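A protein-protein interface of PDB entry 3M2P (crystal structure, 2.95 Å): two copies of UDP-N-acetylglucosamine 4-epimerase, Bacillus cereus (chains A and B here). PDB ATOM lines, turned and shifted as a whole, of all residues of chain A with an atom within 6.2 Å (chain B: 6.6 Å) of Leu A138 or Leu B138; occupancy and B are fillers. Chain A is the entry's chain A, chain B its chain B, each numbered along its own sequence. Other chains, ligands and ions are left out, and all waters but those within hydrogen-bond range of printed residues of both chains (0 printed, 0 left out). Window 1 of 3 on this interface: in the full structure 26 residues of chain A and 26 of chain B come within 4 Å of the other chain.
Leu A138 touches two residues of chain B. Leu B138 touches one residue of chain A. Of the printed residues of chain A, His B142 touches Pro A127 (3.6 Å), Pro A129 (3.8 Å), Val A135 (3.9 Å) and Leu A138 (3.6 Å). Of the printed residues of chain A, Ala B139 touches Val A135. Of the printed residues of chain B, Val A135 touches Ala B139 and His B142. Glu A141 touches none of the printed residues of chain B. Cys B140 touches none of the printed residues of chain A. The nearest residue of chain B that does not touch Leu A138 is Val B135 (5.5 Å). The nearest residue of chain A that does not touch Leu B138 is His A142 (4.8 Å).
The backbone NH (N) of Leu B128 sits at hydrogen-bond distance from the backbone carbonyl oxygen (O) of Ala B112. OD1 of Asn B145 is in hydrogen-bond range of ND1 of His B142, at 3.4 Å.
Hydrophobic or aromatic side chains of chain B within 4 Å of the printed part of chain A: Pro B129, Val B135, Leu B138 and His B142. Of the 18 printed residues of chain A, 6 touch a printed residue of chain B. Hydrophobic or aromatic side chains of chain A within 4 Å of the printed part of chain B: Pro A129, Val A135, Leu A138 and His A142. Among the printed residues, 10 pairs touch across the chains.
Pro A127 touches His B142, and with the chains exchanged His A142 touches Pro B127. Pro A129 touches His B142, and with the chains exchanged His A142 touches Pro B129. Val A135 touches Ala B139, and with the chains exchanged Ala A139 touches Val B135. Val A135 touches His B142, but with the chains exchanged His A142 does not touch Val B135 (4.3 Å). Of the 10 pairs that touch across the chains among the printed residues, 7 have their exchanged pair printed and touching as well.
CE1 of His B142 touches O of Pro A127 (3.6 Å). His B142 touches Pro A129. Val A135 touches Ala B139 (CG1 to O, 3.8 Å). Val A135 touches His B142. Leu A138 touches Leu B138. Leu A138 touches His B142. Val B135 touches Ala A139 (CG1 to O, 3.7 Å). CE1 of His A142 touches O of Pro B127, at 3.4 Å. CE1 of His A142 touches CA of Leu B128, 3.99 Å away. His A142 touches Pro B129 (ND1 to CD, 3.0 Å).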
ATOM      1  N   TYR A 106      20.429  21.226  -4.463  1.00  0.00           N
ATOM      2  CA  TYR A 106      21.427  20.351  -3.847  1.00  0.00           C
ATOM      3  C   TYR A 106      20.755  19.229  -3.096  1.00  0.00           C
ATOM      4  O   TYR A 106      19.760  19.458  -2.420  1.00  0.00           O
ATOM      5  CB  TYR A 106      22.319  21.117  -2.866  1.00  0.00           C
ATOM      6  CG  TYR A 106      23.310  20.221  -2.162  1.00  0.00           C
ATOM      7  CD1 TYR A 106      24.335  19.603  -2.873  1.00  0.00           C
ATOM      8  CD2 TYR A 106      23.216  19.974  -0.801  1.00  0.00           C
ATOM      9  CE1 TYR A 106      25.245  18.782  -2.253  1.00  0.00           C
ATOM     10  CE2 TYR A 106      24.121  19.146  -0.171  1.00  0.00           C
ATOM     11  CZ  TYR A 106      25.138  18.556  -0.904  1.00  0.00           C
ATOM     12  OH  TYR A 106      26.051  17.725  -0.292  1.00  0.00           O
ATOM     13  N   SER A 108      20.714  17.213  -0.017  1.00  0.00           N
ATOM     14  CA  SER A 108      21.176  16.995   1.349  1.00  0.00           C
ATOM     15  C   SER A 108      20.440  15.799   1.975  1.00  0.00           C
ATOM     16  O   SER A 108      19.847  14.984   1.256  1.00  0.00           O
ATOM     17  CB  SER A 108      21.005  18.250   2.191  1.00  0.00           C
ATOM     18  OG  SER A 108      21.798  18.187   3.358  1.00  0.00           O
ATOM     19  N   ALA A 112      21.395  14.916   8.733  1.00  0.00           N
ATOM     20  CA  ALA A 112      21.915  16.138   9.335  1.00  0.00           C
ATOM     21  C   ALA A 112      21.331  16.242  10.730  1.00  0.00           C
ATOM     22  O   ALA A 112      21.674  17.141  11.491  1.00  0.00           O
ATOM     23  CB  ALA A 112      21.524  17.351   8.514  1.00  0.00           C
ATOM     24  N   PRO A 127      21.344  21.054  13.443  1.00  0.00           N
ATOM     25  CA  PRO A 127      21.902  19.848  12.836  1.00  0.00           C
ATOM     26  C   PRO A 127      22.848  19.206  13.833  1.00  0.00           C
ATOM     27  O   PRO A 127      23.480  19.900  14.616  1.00  0.00           O
ATOM     28  CB  PRO A 127      22.667  20.386  11.623  1.00  0.00           C
ATOM     29  CG  PRO A 127      22.048  21.696  11.335  1.00  0.00           C
ATOM     30  CD  PRO A 127      21.656  22.264  12.666  1.00  0.00           C
ATOM     31  N   LEU A 128      22.924  17.888  13.821  1.00  0.00           N
ATOM     32  CA  LEU A 128      23.769  17.168  14.755  1.00  0.00           C
ATOM     33  C   LEU A 128      23.954  15.767  14.196  1.00  0.00           C
ATOM     34  O   LEU A 128      23.229  14.838  14.565  1.00  0.00           O
ATOM     35  CB  LEU A 128      23.136  17.153  16.146  1.00  0.00           C
ATOM     36  CG  LEU A 128      23.646  16.240  17.250  1.00  0.00           C
ATOM     37  CD1 LEU A 128      23.565  16.971  18.554  1.00  0.00           C
ATOM     38  CD2 LEU A 128      22.795  14.990  17.319  1.00  0.00           C
ATOM     39  N   PRO A 129      24.913  15.628  13.272  1.00  0.00           N
ATOM     40  CA  PRO A 129      25.096  14.403  12.504  1.00  0.00           C
ATOM     41  C   PRO A 129      25.768  13.347  13.362  1.00  0.00           C
ATOM     42  O   PRO A 129      26.504  13.686  14.288  1.00  0.00           O
ATOM     43  CB  PRO A 129      26.025  14.838  11.359  1.00  0.00           C
ATOM     44  CG  PRO A 129      26.085  16.336  11.425  1.00  0.00           C
ATOM     45  CD  PRO A 129      25.845  16.684  12.850  1.00  0.00           C
ATOM     46  N   TYR A 133      29.620  11.246   6.951  1.00  0.00           N
ATOM     47  CA  TYR A 133      28.749  11.559   5.815  1.00  0.00           C
ATOM     48  C   TYR A 133      27.855  12.766   6.104  1.00  0.00           C
ATOM     49  O   TYR A 133      27.732  13.671   5.281  1.00  0.00           O
ATOM     50  CB  TYR A 133      27.913  10.328   5.445  1.00  0.00           C
ATOM     51  CG  TYR A 133      26.694  10.564   4.578  1.00  0.00           C
ATOM     52  CD1 TYR A 133      26.804  10.770   3.205  1.00  0.00           C
ATOM     53  CD2 TYR A 133      25.421  10.529   5.129  1.00  0.00           C
ATOM     54  CE1 TYR A 133      25.669  10.971   2.412  1.00  0.00           C
ATOM     55  CE2 TYR A 133      24.285  10.721   4.354  1.00  0.00           C
ATOM     56  CZ  TYR A 133      24.408  10.937   3.000  1.00  0.00           C
ATOM     57  OH  TYR A 133      23.256  11.123   2.253  1.00  0.00           O
ATOM     58  N   GLY A 134      27.250  12.778   7.282  1.00  0.00           N
ATOM     59  CA  GLY A 134      26.393  13.871   7.684  1.00  0.00           C
ATOM     60  C   GLY A 134      27.152  15.171   7.750  1.00  0.00           C
ATOM     61  O   GLY A 134      26.797  16.136   7.078  1.00  0.00           O
ATOM     62  N   VAL A 135      28.196  15.208   8.565  1.00  0.00           N
ATOM     63  CA  VAL A 135      29.029  16.406   8.665  1.00  0.00           C
ATOM     64  C   VAL A 135      29.311  17.012   7.294  1.00  0.00           C
ATOM     65  O   VAL A 135      29.111  18.205   7.082  1.00  0.00           O
ATOM     66  CB  VAL A 135      30.365  16.114   9.355  1.00  0.00           C
ATOM     67  CG1 VAL A 135      31.099  17.408   9.602  1.00  0.00           C
ATOM     68  CG2 VAL A 135      30.130  15.378  10.665  1.00  0.00           C
ATOM     69  N   SER A 136      29.765  16.178   6.363  1.00  0.00           N
ATOM     70  CA  SER A 136      30.090  16.629   5.010  1.00  0.00           C
ATOM     71  C   SER A 136      28.905  17.272   4.304  1.00  0.00           C
ATOM     72  O   SER A 136      29.002  18.387   3.817  1.00  0.00           O
ATOM     73  CB  SER A 136      30.614  15.466   4.157  1.00  0.00           C
ATOM     74  OG  SER A 136      31.067  15.936   2.895  1.00  0.00           O
ATOM     75  N   LYS A 137      27.800  16.543   4.225  1.00  0.00           N
ATOM     76  CA  LYS A 137      26.597  17.036   3.577  1.00  0.00           C
ATOM     77  C   LYS A 137      26.259  18.407   4.141  1.00  0.00           C
ATOM     78  O   LYS A 137      25.995  19.358   3.399  1.00  0.00           O
ATOM     79  CB  LYS A 137      25.444  16.059   3.800  1.00  0.00           C
ATOM     80  CG  LYS A 137      25.444  14.881   2.848  1.00  0.00           C
ATOM     81  CD  LYS A 137      25.083  15.345   1.469  1.00  0.00           C
ATOM     82  CE  LYS A 137      25.431  14.313   0.429  1.00  0.00           C
ATOM     83  NZ  LYS A 137      25.828  14.975  -0.864  1.00  0.00           N
ATOM     84  N   LEU A 138      26.291  18.496   5.464  1.00  0.00           N
ATOM     85  CA  LEU A 138      26.064  19.745   6.179  1.00  0.00           C
ATOM     86  C   LEU A 138      27.029  20.864   5.734  1.00  0.00           C
ATOM     87  O   LEU A 138      26.673  22.034   5.731  1.00  0.00           O
ATOM     88  CB  LEU A 138      26.196  19.476   7.681  1.00  0.00           C
ATOM     89  CG  LEU A 138      25.598  20.385   8.755  1.00  0.00           C
ATOM     90  CD1 LEU A 138      25.956  19.815  10.111  1.00  0.00           C
ATOM     91  CD2 LEU A 138      26.115  21.803   8.656  1.00  0.00           C
ATOM     92  N   ALA A 139      28.254  20.500   5.374  1.00  0.00           N
ATOM     93  CA  ALA A 139      29.262  21.478   4.954  1.00  0.00           C
ATOM     94  C   ALA A 139      28.960  22.011   3.556  1.00  0.00           C
ATOM     95  O   ALA A 139      29.067  23.213   3.304  1.00  0.00           O
ATOM     96  CB  ALA A 139      30.642  20.858   4.996  1.00  0.00           C
ATOM     97  N   CYS A 140      28.577  21.111   2.653  1.00  0.00           N
ATOM     98  CA  CYS A 140      28.223  21.482   1.288  1.00  0.00           C
ATOM     99  C   CYS A 140      26.977  22.370   1.259  1.00  0.00           C
ATOM    100  O   CYS A 140      26.818  23.196   0.361  1.00  0.00           O
ATOM    101  CB  CYS A 140      28.007  20.235   0.433  1.00  0.00           C
ATOM    102  SG  CYS A 140      29.481  19.219   0.181  1.00  0.00           S
ATOM    103  N   GLU A 141      26.091  22.179   2.238  1.00  0.00           N
ATOM    104  CA  GLU A 141      24.906  23.012   2.402  1.00  0.00           C
ATOM    105  C   GLU A 141      25.273  24.467   2.634  1.00  0.00           C
ATOM    106  O   GLU A 141      24.716  25.361   2.008  1.00  0.00           O
ATOM    107  CB  GLU A 141      24.096  22.543   3.593  1.00  0.00           C
ATOM    108  CG  GLU A 141      23.112  21.450   3.305  1.00  0.00           C
ATOM    109  CD  GLU A 141      22.162  21.283   4.469  1.00  0.00           C
ATOM    110  OE1 GLU A 141      22.109  22.236   5.281  1.00  0.00           O
ATOM    111  OE2 GLU A 141      21.488  20.227   4.577  1.00  0.00           O
ATOM    112  N   HIS A 142      26.202  24.699   3.551  1.00  0.00           N
ATOM    113  CA  HIS A 142      26.668  26.046   3.829  1.00  0.00           C
ATOM    114  C   HIS A 142      27.566  26.622   2.729  1.00  0.00           C
ATOM    115  O   HIS A 142      27.610  27.839   2.526  1.00  0.00           O
ATOM    116  CB  HIS A 142      27.323  26.099   5.201  1.00  0.00           C
ATOM    117  CG  HIS A 142      26.342  25.940   6.315  1.00  0.00           C
ATOM    118  ND1 HIS A 142      25.515  26.964   6.727  1.00  0.00           N
ATOM    119  CD2 HIS A 142      26.019  24.867   7.077  1.00  0.00           C
ATOM    120  CE1 HIS A 142      24.742  26.535   7.709  1.00  0.00           C
ATOM    121  NE2 HIS A 142      25.026  25.266   7.938  1.00  0.00           N
ATOM    122  N   ILE A 143      28.268  25.758   2.005  1.00  0.00           N
ATOM    123  CA  ILE A 143      28.965  26.216   0.813  1.00  0.00           C
ATOM    124  C   ILE A 143      27.957  26.892  -0.125  1.00  0.00           C
ATOM    125  O   ILE A 143      28.160  28.029  -0.560  1.00  0.00           O
ATOM    126  CB  ILE A 143      29.705  25.073   0.092  1.00  0.00           C
ATOM    127  CG1 ILE A 143      30.881  24.593   0.954  1.00  0.00           C
ATOM    128  CG2 ILE A 143      30.167  25.523  -1.296  1.00  0.00           C
ATOM    129  CD1 ILE A 143      31.724  23.494   0.326  1.00  0.00           C
ATOM    130  N   ARG A 159      16.913  18.388   2.181  1.00  0.00           N
ATOM    131  CA  ARG A 159      17.218  17.292   3.101  1.00  0.00           C
ATOM    132  C   ARG A 159      16.276  16.088   2.916  1.00  0.00           C
ATOM    133  O   ARG A 159      15.274  15.966   3.617  1.00  0.00           O
ATOM    134  CB  ARG A 159      17.209  17.783   4.548  1.00  0.00           C
ATOM    135  CG  ARG A 159      18.292  18.784   4.824  1.00  0.00           C
ATOM    136  CD  ARG A 159      18.195  19.364   6.204  1.00  0.00           C
ATOM    137  NE  ARG A 159      19.366  20.182   6.507  1.00  0.00           N
ATOM    138  CZ  ARG A 159      19.401  21.120   7.451  1.00  0.00           C
ATOM    139  NH1 ARG A 159      18.322  21.375   8.186  1.00  0.00           N
ATOM    140  NH2 ARG A 159      20.516  21.807   7.668  1.00  0.00           N
ATOM    141  N   TYR B 106      38.381  22.586  22.290  1.00  0.00           N
ATOM    142  CA  TYR B 106      38.560  22.985  20.896  1.00  0.00           C
ATOM    143  C   TYR B 106      38.376  24.488  20.673  1.00  0.00           C
ATOM    144  O   TYR B 106      37.445  25.090  21.208  1.00  0.00           O
ATOM    145  CB  TYR B 106      37.590  22.219  20.002  1.00  0.00           C
ATOM    146  CG  TYR B 106      37.669  22.629  18.553  1.00  0.00           C
ATOM    147  CD1 TYR B 106      38.873  22.563  17.862  1.00  0.00           C
ATOM    148  CD2 TYR B 106      36.541  23.081  17.864  1.00  0.00           C
ATOM    149  CE1 TYR B 106      38.955  22.934  16.526  1.00  0.00           C
ATOM    150  CE2 TYR B 106      36.620  23.456  16.524  1.00  0.00           C
ATOM    151  CZ  TYR B 106      37.832  23.372  15.870  1.00  0.00           C
ATOM    152  OH  TYR B 106      37.941  23.730  14.559  1.00  0.00           O
ATOM    153  N   SER B 108      36.950  26.908  18.544  1.00  0.00           N
ATOM    154  CA  SER B 108      36.004  27.246  17.496  1.00  0.00           C
ATOM    155  C   SER B 108      35.849  28.756  17.455  1.00  0.00           C
ATOM    156  O   SER B 108      36.573  29.471  18.141  1.00  0.00           O
ATOM    157  CB  SER B 108      34.656  26.588  17.754  1.00  0.00           C
ATOM    158  OG  SER B 108      33.829  26.717  16.617  1.00  0.00           O
ATOM    159  N   ALA B 112      30.814  31.071  13.470  1.00  0.00           N
ATOM    160  CA  ALA B 112      29.816  30.046  13.181  1.00  0.00           C
ATOM    161  C   ALA B 112      28.480  30.718  12.904  1.00  0.00           C
ATOM    162  O   ALA B 112      27.640  30.196  12.179  1.00  0.00           O
ATOM    163  CB  ALA B 112      29.683  29.080  14.345  1.00  0.00           C
ATOM    164  N   PRO B 127      23.568  27.722  13.183  1.00  0.00           N
ATOM    165  CA  PRO B 127      24.825  28.184  12.586  1.00  0.00           C
ATOM    166  C   PRO B 127      24.588  28.642  11.161  1.00  0.00           C
ATOM    167  O   PRO B 127      23.696  28.119  10.484  1.00  0.00           O
ATOM    168  CB  PRO B 127      25.686  26.920  12.563  1.00  0.00           C
ATOM    169  CG  PRO B 127      25.129  26.043  13.615  1.00  0.00           C
ATOM    170  CD  PRO B 127      23.651  26.318  13.621  1.00  0.00           C
ATOM    171  N   LEU B 128      25.381  29.605  10.712  1.00  0.00           N
ATOM    172  CA  LEU B 128      25.261  30.131   9.362  1.00  0.00           C
ATOM    173  C   LEU B 128      26.597  30.752   8.955  1.00  0.00           C
ATOM    174  O   LEU B 128      26.730  31.973   8.899  1.00  0.00           O
ATOM    175  CB  LEU B 128      24.128  31.157   9.296  1.00  0.00           C
ATOM    176  CG  LEU B 128      23.634  31.593   7.919  1.00  0.00           C
ATOM    177  CD1 LEU B 128      22.856  30.492   7.253  1.00  0.00           C
ATOM    178  CD2 LEU B 128      22.795  32.836   8.034  1.00  0.00           C
ATOM    179  N   PRO B 129      27.593  29.902   8.670  1.00  0.00           N
ATOM    180  CA  PRO B 129      28.942  30.402   8.388  1.00  0.00           C
ATOM    181  C   PRO B 129      28.944  31.371   7.199  1.00  0.00           C
ATOM    182  O   PRO B 129      28.194  31.202   6.240  1.00  0.00           O
ATOM    183  CB  PRO B 129      29.734  29.130   8.051  1.00  0.00           C
ATOM    184  CG  PRO B 129      28.891  27.996   8.509  1.00  0.00           C
ATOM    185  CD  PRO B 129      27.476  28.457   8.424  1.00  0.00           C
ATOM    186  N   TYR B 133      36.165  29.505   6.219  1.00  0.00           N
ATOM    187  CA  TYR B 133      36.840  29.396   7.495  1.00  0.00           C
ATOM    188  C   TYR B 133      35.894  28.852   8.552  1.00  0.00           C
ATOM    189  O   TYR B 133      36.249  27.945   9.313  1.00  0.00           O
ATOM    190  CB  TYR B 133      37.356  30.761   7.929  1.00  0.00           C
ATOM    191  CG  TYR B 133      37.736  30.804   9.378  1.00  0.00           C
ATOM    192  CD1 TYR B 133      38.846  30.121   9.836  1.00  0.00           C
ATOM    193  CD2 TYR B 133      36.982  31.522  10.289  1.00  0.00           C
ATOM    194  CE1 TYR B 133      39.201  30.156  11.160  1.00  0.00           C
ATOM    195  CE2 TYR B 133      37.321  31.562  11.617  1.00  0.00           C
ATOM    196  CZ  TYR B 133      38.438  30.878  12.048  1.00  0.00           C
ATOM    197  OH  TYR B 133      38.789  30.912  13.376  1.00  0.00           O
ATOM    198  N   GLY B 134      34.690  29.422   8.589  1.00  0.00           N
ATOM    199  CA  GLY B 134      33.687  29.081   9.582  1.00  0.00           C
ATOM    200  C   GLY B 134      32.998  27.771   9.277  1.00  0.00           C
ATOM    201  O   GLY B 134      32.709  27.004  10.188  1.00  0.00           O
ATOM    202  N   VAL B 135      32.735  27.515   8.002  1.00  0.00           N
ATOM    203  CA  VAL B 135      32.156  26.248   7.580  1.00  0.00           C
ATOM    204  C   VAL B 135      32.963  25.080   8.121  1.00  0.00           C
ATOM    205  O   VAL B 135      32.410  24.086   8.589  1.00  0.00           O
ATOM    206  CB  VAL B 135      32.140  26.134   6.050  1.00  0.00           C
ATOM    207  CG1 VAL B 135      31.442  24.857   5.603  1.00  0.00           C
ATOM    208  CG2 VAL B 135      31.470  27.348   5.445  1.00  0.00           C
ATOM    209  N   SER B 136      34.277  25.209   8.051  1.00  0.00           N
ATOM    210  CA  SER B 136      35.180  24.134   8.418  1.00  0.00           C
ATOM    211  C   SER B 136      35.342  24.046   9.929  1.00  0.00           C
ATOM    212  O   SER B 136      35.687  22.997  10.474  1.00  0.00           O
ATOM    213  CB  SER B 136      36.544  24.357   7.759  1.00  0.00           C
ATOM    214  OG  SER B 136      37.498  23.446   8.263  1.00  0.00           O
ATOM    215  N   LYS B 137      35.117  25.166  10.600  1.00  0.00           N
ATOM    216  CA  LYS B 137      35.186  25.204  12.045  1.00  0.00           C
ATOM    217  C   LYS B 137      33.962  24.479  12.577  1.00  0.00           C
ATOM    218  O   LYS B 137      34.026  23.798  13.595  1.00  0.00           O
ATOM    219  CB  LYS B 137      35.220  26.649  12.538  1.00  0.00           C
ATOM    220  CG  LYS B 137      36.588  27.279  12.486  1.00  0.00           C
ATOM    221  CD  LYS B 137      37.402  26.844  13.677  1.00  0.00           C
ATOM    222  CE  LYS B 137      38.883  27.012  13.433  1.00  0.00           C
ATOM    223  NZ  LYS B 137      39.671  26.022  14.244  1.00  0.00           N
ATOM    224  N   LEU B 138      32.845  24.630  11.873  1.00  0.00           N
ATOM    225  CA  LEU B 138      31.613  23.950  12.225  1.00  0.00           C
ATOM    226  C   LEU B 138      31.810  22.465  12.005  1.00  0.00           C
ATOM    227  O   LEU B 138      31.390  21.638  12.806  1.00  0.00           O
ATOM    228  CB  LEU B 138      30.466  24.478  11.368  1.00  0.00           C
ATOM    229  CG  LEU B 138      29.044  24.001  11.687  1.00  0.00           C
ATOM    230  CD1 LEU B 138      28.117  25.188  11.788  1.00  0.00           C
ATOM    231  CD2 LEU B 138      28.498  22.962  10.670  1.00  0.00           C
ATOM    232  N   ALA B 139      32.479  22.132  10.912  1.00  0.00           N
ATOM    233  CA  ALA B 139      32.816  20.748  10.619  1.00  0.00           C
ATOM    234  C   ALA B 139      33.651  20.101  11.740  1.00  0.00           C
ATOM    235  O   ALA B 139      33.314  19.022  12.216  1.00  0.00           O
ATOM    236  CB  ALA B 139      33.526  20.652   9.287  1.00  0.00           C
ATOM    237  N   CYS B 140      34.730  20.763  12.158  1.00  0.00           N
ATOM    238  CA  CYS B 140      35.571  20.266  13.248  1.00  0.00           C
ATOM    239  C   CYS B 140      34.808  20.170  14.568  1.00  0.00           C
ATOM    240  O   CYS B 140      35.156  19.369  15.444  1.00  0.00           O
ATOM    241  CB  CYS B 140      36.806  21.154  13.445  1.00  0.00           C
ATOM    242  SG  CYS B 140      38.052  21.106  12.117  1.00  0.00           S
ATOM    243  N   GLU B 141      33.780  20.998  14.725  1.00  0.00           N
ATOM    244  CA  GLU B 141      32.946  20.929  15.918  1.00  0.00           C
ATOM    245  C   GLU B 141      32.210  19.592  15.951  1.00  0.00           C
ATOM    246  O   GLU B 141      32.210  18.882  16.961  1.00  0.00           O
ATOM    247  CB  GLU B 141      31.946  22.075  15.944  1.00  0.00           C
ATOM    248  CG  GLU B 141      32.506  23.385  16.414  1.00  0.00           C
ATOM    249  CD  GLU B 141      31.413  24.343  16.802  1.00  0.00           C
ATOM    250  OE1 GLU B 141      30.241  23.956  16.708  1.00  0.00           O
ATOM    251  OE2 GLU B 141      31.710  25.477  17.211  1.00  0.00           O
ATOM    252  N   HIS B 142      31.589  19.251  14.828  1.00  0.00           N
ATOM    253  CA  HIS B 142      30.813  18.028  14.737  1.00  0.00           C
ATOM    254  C   HIS B 142      31.688  16.785  14.763  1.00  0.00           C
ATOM    255  O   HIS B 142      31.232  15.710  15.159  1.00  0.00           O
ATOM    256  CB  HIS B 142      29.895  18.077  13.516  1.00  0.00           C
ATOM    257  CG  HIS B 142      28.763  19.051  13.671  1.00  0.00           C
ATOM    258  ND1 HIS B 142      28.009  19.135  14.826  1.00  0.00           N
ATOM    259  CD2 HIS B 142      28.264  19.985  12.826  1.00  0.00           C
ATOM    260  CE1 HIS B 142      27.095  20.077  14.681  1.00  0.00           C
ATOM    261  NE2 HIS B 142      27.231  20.612  13.480  1.00  0.00           N
ATOM    262  N   ILE B 143      32.953  16.937  14.370  1.00  0.00           N
ATOM    263  CA  ILE B 143      33.931  15.853  14.500  1.00  0.00           C
ATOM    264  C   ILE B 143      34.125  15.573  15.987  1.00  0.00           C
ATOM    265  O   ILE B 143      34.053  14.424  16.433  1.00  0.00           O
ATOM    266  CB  ILE B 143      35.293  16.176  13.839  1.00  0.00           C
ATOM    267  CG1 ILE B 143      35.133  16.404  12.343  1.00  0.00           C
ATOM    268  CG2 ILE B 143      36.255  15.027  14.036  1.00  0.00           C
ATOM    269  CD1 ILE B 143      36.436  16.485  11.593  1.00  0.00           C
ATOM    270  N   ASN B 145      32.013  16.339  18.295  1.00  0.00           N
ATOM    271  CA  ASN B 145      30.760  15.904  18.874  1.00  0.00           C
ATOM    272  C   ASN B 145      30.555  14.412  18.688  1.00  0.00           C
ATOM    273  O   ASN B 145      30.359  13.684  19.658  1.00  0.00           O
ATOM    274  CB  ASN B 145      29.592  16.691  18.288  1.00  0.00           C
ATOM    275  CG  ASN B 145      29.593  18.136  18.734  1.00  0.00           C
ATOM    276  OD1 ASN B 145      28.958  18.996  18.112  1.00  0.00           O
ATOM    277  ND2 ASN B 145      30.314  18.415  19.820  1.00  0.00           N
ATOM    278  N   ARG B 159      33.556  28.523  21.495  1.00  0.00           N
ATOM    279  CA  ARG B 159      33.308  29.430  20.378  1.00  0.00           C
ATOM    280  C   ARG B 159      33.743  30.844  20.739  1.00  0.00           C
ATOM    281  O   ARG B 159      32.941  31.659  21.214  1.00  0.00           O
ATOM    282  CB  ARG B 159      31.834  29.411  19.964  1.00  0.00           C
ATOM    283  CG  ARG B 159      31.429  28.222  19.109  1.00  0.00           C
ATOM    284  CD  ARG B 159      29.958  28.309  18.675  1.00  0.00           C
ATOM    285  NE  ARG B 159      29.566  27.204  17.798  1.00  0.00           N
ATOM    286  CZ  ARG B 159      28.308  26.877  17.522  1.00  0.00           C
ATOM    287  NH1 ARG B 159      27.304  27.563  18.056  1.00  0.00           N
ATOM    288  NH2 ARG B 159      28.050  25.861  16.714  1.00  0.00           N
